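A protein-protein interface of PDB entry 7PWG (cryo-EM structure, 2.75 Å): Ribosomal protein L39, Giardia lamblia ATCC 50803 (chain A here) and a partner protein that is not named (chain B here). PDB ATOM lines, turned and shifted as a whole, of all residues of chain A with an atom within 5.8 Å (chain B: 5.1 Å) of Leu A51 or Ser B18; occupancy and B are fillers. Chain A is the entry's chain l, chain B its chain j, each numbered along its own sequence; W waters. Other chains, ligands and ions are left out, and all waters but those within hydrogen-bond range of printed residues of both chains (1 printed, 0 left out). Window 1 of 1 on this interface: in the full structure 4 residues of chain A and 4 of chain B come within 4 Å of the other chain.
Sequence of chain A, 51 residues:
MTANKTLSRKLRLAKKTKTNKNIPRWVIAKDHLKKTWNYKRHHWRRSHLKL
Hydrophobic or aromatic side chains of chain B within 4 Å of the printed part of chain A: His B25.
Hydrophobic or aromatic side chains of chain A within 4 Å of the printed part of chain B: Leu A51.
Among the printed residues, 4 pairs touch across the chains.
Among the printed residues, pairs that only touch across the chains: Arg A12 with Gly B23 (3.5 Å), Lys A50 with His B25 (3.5 Å) and Leu A51 with Ser B18 (3.6 Å).
The guanidinium group of Arg A9 lies within salt-bridge range of the chain-end carboxylate of Leu A51.
O of His B16 is in hydrogen-bond range of NE2 of His B25 (3.2 Å).
Of chain B, only Ser B18 comes within 4 Å of Leu A51.
Ser B18 touches two residues of chain A.
Printed residues of chain A within 4 Å of His B25: Lys A50.
Of the printed residues of chain A, Gly B23 touches Arg A12 (3.5 Å).
Of the printed residues of chain B, Lys A50 touches His B25.
Lys A16 touches none of the printed residues of chain B.
Arg A9 touches none of the printed residues of chain B.
The nearest printed residue of chain B that does not touch Leu A51 is His B25 (5.3 Å).
The nearest printed residue of chain A that does not touch Gly B23 is Leu A51 (5.6 Å).
Water W1 lies within hydrogen-bond range of the guanidinium group of Arg A12 (2.9 Å) and the backbone carbonyl oxygen of Cys B19 (2.9 Å).
The side-chain hydroxyl (OG) of Ser B18 is in hydrogen-bond range of the guanidinium group (NH1) of Arg A12 (3.2 Å).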
ATOM      1  N   ARG A   9     -21.815 -19.395   9.113  1.00  0.00           N
ATOM      2  CA  ARG A   9     -22.980 -20.272   9.131  1.00  0.00           C
ATOM      3  C   ARG A   9     -22.817 -21.401  10.132  1.00  0.00           C
ATOM      4  O   ARG A   9     -23.802 -21.845  10.726  1.00  0.00           O
ATOM      5  CB  ARG A   9     -23.251 -20.840   7.745  1.00  0.00           C
ATOM      6  CG  ARG A   9     -23.733 -19.834   6.726  1.00  0.00           C
ATOM      7  CD  ARG A   9     -24.019 -20.508   5.391  1.00  0.00           C
ATOM      8  NE  ARG A   9     -25.183 -21.384   5.442  1.00  0.00           N
ATOM      9  CZ  ARG A   9     -25.401 -22.398   4.610  1.00  0.00           C
ATOM     10  NH1 ARG A   9     -26.490 -23.140   4.737  1.00  0.00           N
ATOM     11  NH2 ARG A   9     -24.529 -22.680   3.660  1.00  0.00           N
ATOM     12  N   ARG A  12     -23.905 -20.058  13.735  1.00  0.00           N
ATOM     13  CA  ARG A  12     -25.330 -19.919  13.993  1.00  0.00           C
ATOM     14  C   ARG A  12     -26.029 -21.273  14.046  1.00  0.00           C
ATOM     15  O   ARG A  12     -26.968 -21.446  14.826  1.00  0.00           O
ATOM     16  CB  ARG A  12     -25.964 -19.004  12.953  1.00  0.00           C
ATOM     17  CG  ARG A  12     -25.484 -17.573  13.052  1.00  0.00           C
ATOM     18  CD  ARG A  12     -26.373 -16.612  12.307  1.00  0.00           C
ATOM     19  NE  ARG A  12     -27.685 -16.481  12.920  1.00  0.00           N
ATOM     20  CZ  ARG A  12     -28.604 -15.610  12.536  1.00  0.00           C
ATOM     21  NH1 ARG A  12     -28.356 -14.785  11.539  1.00  0.00           N
ATOM     22  NH2 ARG A  12     -29.772 -15.564  13.147  1.00  0.00           N
ATOM     23  N   LEU A  13     -25.588 -22.239  13.242  1.00  0.00           N
ATOM     24  CA  LEU A  13     -26.080 -23.606  13.379  1.00  0.00           C
ATOM     25  C   LEU A  13     -25.680 -24.209  14.716  1.00  0.00           C
ATOM     26  O   LEU A  13     -26.443 -24.975  15.307  1.00  0.00           O
ATOM     27  CB  LEU A  13     -25.559 -24.482  12.245  1.00  0.00           C
ATOM     28  CG  LEU A  13     -26.160 -24.309  10.857  1.00  0.00           C
ATOM     29  CD1 LEU A  13     -25.566 -25.321   9.916  1.00  0.00           C
ATOM     30  CD2 LEU A  13     -27.660 -24.427  10.904  1.00  0.00           C
ATOM     31  N   LYS A  16     -28.236 -23.230  17.528  1.00  0.00           N
ATOM     32  CA  LYS A  16     -29.507 -23.945  17.525  1.00  0.00           C
ATOM     33  C   LYS A  16     -29.363 -25.355  18.081  1.00  0.00           C
ATOM     34  O   LYS A  16     -30.312 -25.886  18.654  1.00  0.00           O
ATOM     35  CB  LYS A  16     -30.091 -24.004  16.116  1.00  0.00           C
ATOM     36  CG  LYS A  16     -30.359 -22.667  15.477  1.00  0.00           C
ATOM     37  CD  LYS A  16     -31.548 -21.976  16.090  1.00  0.00           C
ATOM     38  CE  LYS A  16     -32.843 -22.621  15.693  1.00  0.00           C
ATOM     39  NZ  LYS A  16     -33.978 -22.025  16.471  1.00  0.00           N
ATOM     40  N   LEU A  49     -34.889 -24.747   9.572  1.00  0.00           N
ATOM     41  CA  LEU A  49     -33.867 -23.779   9.942  1.00  0.00           C
ATOM     42  C   LEU A  49     -33.354 -23.107   8.681  1.00  0.00           C
ATOM     43  O   LEU A  49     -32.822 -23.778   7.794  1.00  0.00           O
ATOM     44  CB  LEU A  49     -32.705 -24.455  10.665  1.00  0.00           C
ATOM     45  CG  LEU A  49     -32.648 -24.687  12.164  1.00  0.00           C
ATOM     46  CD1 LEU A  49     -33.905 -25.309  12.684  1.00  0.00           C
ATOM     47  CD2 LEU A  49     -31.463 -25.566  12.450  1.00  0.00           C
ATOM     48  N   LYS A  50     -33.540 -21.808   8.556  1.00  0.00           N
ATOM     49  CA  LYS A  50     -33.048 -21.095   7.382  1.00  0.00           C
ATOM     50  C   LYS A  50     -31.753 -20.363   7.717  1.00  0.00           C
ATOM     51  O   LYS A  50     -31.644 -19.147   7.634  1.00  0.00           O
ATOM     52  CB  LYS A  50     -34.122 -20.156   6.850  1.00  0.00           C
ATOM     53  CG  LYS A  50     -35.237 -20.888   6.140  1.00  0.00           C
ATOM     54  CD  LYS A  50     -36.416 -19.984   5.854  1.00  0.00           C
ATOM     55  CE  LYS A  50     -37.421 -20.686   4.985  1.00  0.00           C
ATOM     56  NZ  LYS A  50     -38.609 -19.858   4.696  1.00  0.00           N
ATOM     57  N   LEU A  51     -30.763 -21.149   8.119  1.00  0.00           N
ATOM     58  CA  LEU A  51     -29.489 -20.623   8.593  1.00  0.00           C
ATOM     59  C   LEU A  51     -28.309 -21.336   7.929  1.00  0.00           C
ATOM     60  O   LEU A  51     -28.481 -22.220   7.092  1.00  0.00           O
ATOM     61  CB  LEU A  51     -29.388 -20.748  10.117  1.00  0.00           C
ATOM     62  CG  LEU A  51     -30.015 -19.640  10.962  1.00  0.00           C
ATOM     63  CD1 LEU A  51     -29.546 -18.304  10.466  1.00  0.00           C
ATOM     64  CD2 LEU A  51     -31.527 -19.690  10.954  1.00  0.00           C
ATOM     65  OXT LEU A  51     -27.148 -21.042   8.223  1.00  0.00           O
ATOM     66  N   HIS B  16     -31.667 -16.475  -0.814  1.00  0.00           N
ATOM     67  CA  HIS B  16     -31.405 -15.482   0.211  1.00  0.00           C
ATOM     68  C   HIS B  16     -30.549 -16.087   1.311  1.00  0.00           C
ATOM     69  O   HIS B  16     -30.565 -17.296   1.528  1.00  0.00           O
ATOM     70  CB  HIS B  16     -32.715 -14.933   0.796  1.00  0.00           C
ATOM     71  CG  HIS B  16     -33.560 -14.199  -0.197  1.00  0.00           C
ATOM     72  ND1 HIS B  16     -34.433 -14.833  -1.051  1.00  0.00           N
ATOM     73  CD2 HIS B  16     -33.662 -12.883  -0.477  1.00  0.00           C
ATOM     74  CE1 HIS B  16     -35.034 -13.942  -1.812  1.00  0.00           C
ATOM     75  NE2 HIS B  16     -34.587 -12.749  -1.480  1.00  0.00           N
ATOM     76  N   GLY B  17     -29.794 -15.232   1.993  1.00  0.00           N
ATOM     77  CA  GLY B  17     -29.003 -15.613   3.145  1.00  0.00           C
ATOM     78  C   GLY B  17     -29.203 -14.693   4.334  1.00  0.00           C
ATOM     79  O   GLY B  17     -30.159 -13.925   4.358  1.00  0.00           O
ATOM     80  N   SER B  18     -28.323 -14.754   5.326  1.00  0.00           N
ATOM     81  CA  SER B  18     -28.467 -13.939   6.527  1.00  0.00           C
ATOM     82  C   SER B  18     -27.947 -12.527   6.301  1.00  0.00           C
ATOM     83  O   SER B  18     -26.851 -12.340   5.774  1.00  0.00           O
ATOM     84  CB  SER B  18     -27.730 -14.569   7.704  1.00  0.00           C
ATOM     85  OG  SER B  18     -28.543 -15.485   8.389  1.00  0.00           O
ATOM     86  N   CYS B  19     -28.735 -11.540   6.711  1.00  0.00           N
ATOM     87  CA  CYS B  19     -28.323 -10.149   6.638  1.00  0.00           C
ATOM     88  C   CYS B  19     -27.416  -9.797   7.807  1.00  0.00           C
ATOM     89  O   CYS B  19     -27.641 -10.231   8.937  1.00  0.00           O
ATOM     90  CB  CYS B  19     -29.543  -9.232   6.625  1.00  0.00           C
ATOM     91  SG  CYS B  19     -29.174  -7.471   6.513  1.00  0.00           S
ATOM     92  N   ARG B  20     -26.379  -9.014   7.525  1.00  0.00           N
ATOM     93  CA  ARG B  20     -25.459  -8.562   8.555  1.00  0.00           C
ATOM     94  C   ARG B  20     -26.027  -7.442   9.421  1.00  0.00           C
ATOM     95  O   ARG B  20     -25.533  -7.229  10.529  1.00  0.00           O
ATOM     96  CB  ARG B  20     -24.148  -8.101   7.922  1.00  0.00           C
ATOM     97  CG  ARG B  20     -24.219  -6.746   7.285  1.00  0.00           C
ATOM     98  CD  ARG B  20     -22.858  -6.171   7.097  1.00  0.00           C
ATOM     99  NE  ARG B  20     -22.177  -6.786   5.974  1.00  0.00           N
ATOM    100  CZ  ARG B  20     -20.940  -6.495   5.609  1.00  0.00           C
ATOM    101  NH1 ARG B  20     -20.250  -5.602   6.294  1.00  0.00           N
ATOM    102  NH2 ARG B  20     -20.399  -7.097   4.565  1.00  0.00           N
ATOM    103  N   GLY B  23     -30.315  -9.396  10.476  1.00  0.00           N
ATOM    104  CA  GLY B  23     -30.263 -10.767  10.918  1.00  0.00           C
ATOM    105  C   GLY B  23     -31.212 -11.727  10.238  1.00  0.00           C
ATOM    106  O   GLY B  23     -31.184 -12.917  10.558  1.00  0.00           O
ATOM    107  N   LYS B  24     -32.037 -11.266   9.311  1.00  0.00           N
ATOM    108  CA  LYS B  24     -33.085 -12.107   8.756  1.00  0.00           C
ATOM    109  C   LYS B  24     -32.622 -12.818   7.489  1.00  0.00           C
ATOM    110  O   LYS B  24     -31.627 -12.457   6.868  1.00  0.00           O
ATOM    111  CB  LYS B  24     -34.341 -11.284   8.483  1.00  0.00           C
ATOM    112  CG  LYS B  24     -35.012 -10.798   9.753  1.00  0.00           C
ATOM    113  CD  LYS B  24     -36.266 -10.001   9.484  1.00  0.00           C
ATOM    114  CE  LYS B  24     -37.266 -10.781   8.673  1.00  0.00           C
ATOM    115  NZ  LYS B  24     -38.536 -10.051   8.492  1.00  0.00           N
ATOM    116  N   HIS B  25     -33.361 -13.862   7.127  1.00  0.00           N
ATOM    117  CA  HIS B  25     -33.073 -14.686   5.956  1.00  0.00           C
ATOM    118  C   HIS B  25     -33.559 -13.983   4.683  1.00  0.00           C
ATOM    119  O   HIS B  25     -34.392 -14.477   3.933  1.00  0.00           O
ATOM    120  CB  HIS B  25     -33.710 -16.057   6.157  1.00  0.00           C
ATOM    121  CG  HIS B  25     -33.591 -16.977   4.987  1.00  0.00           C
ATOM    122  ND1 HIS B  25     -34.647 -17.239   4.142  1.00  0.00           N
ATOM    123  CD2 HIS B  25     -32.550 -17.702   4.522  1.00  0.00           C
ATOM    124  CE1 HIS B  25     -34.257 -18.078   3.201  1.00  0.00           C
ATOM    125  NE2 HIS B  25     -32.989 -18.371   3.407  1.00  0.00           N
ATOM    126  N   PHE B  27     -31.198 -11.582   2.715  1.00  0.00           N
ATOM    127  CA  PHE B  27     -30.144 -10.962   1.926  1.00  0.00           C
ATOM    128  C   PHE B  27     -29.992 -11.699   0.599  1.00  0.00           C
ATOM    129  O   PHE B  27     -29.607 -12.866   0.577  1.00  0.00           O
ATOM    130  CB  PHE B  27     -28.828 -10.956   2.696  1.00  0.00           C
ATOM    131  CG  PHE B  27     -27.785 -10.094   2.087  1.00  0.00           C
ATOM    132  CD1 PHE B  27     -27.893  -8.723   2.133  1.00  0.00           C
ATOM    133  CD2 PHE B  27     -26.693 -10.649   1.456  1.00  0.00           C
ATOM    134  CE1 PHE B  27     -26.937  -7.933   1.574  1.00  0.00           C
ATOM    135  CE2 PHE B  27     -25.734  -9.855   0.902  1.00  0.00           C
ATOM    136  CZ  PHE B  27     -25.861  -8.495   0.961  1.00  0.00           C
HETATM  137  O   HOH W   1     -26.931 -12.465  10.657  1.00  0.00           O
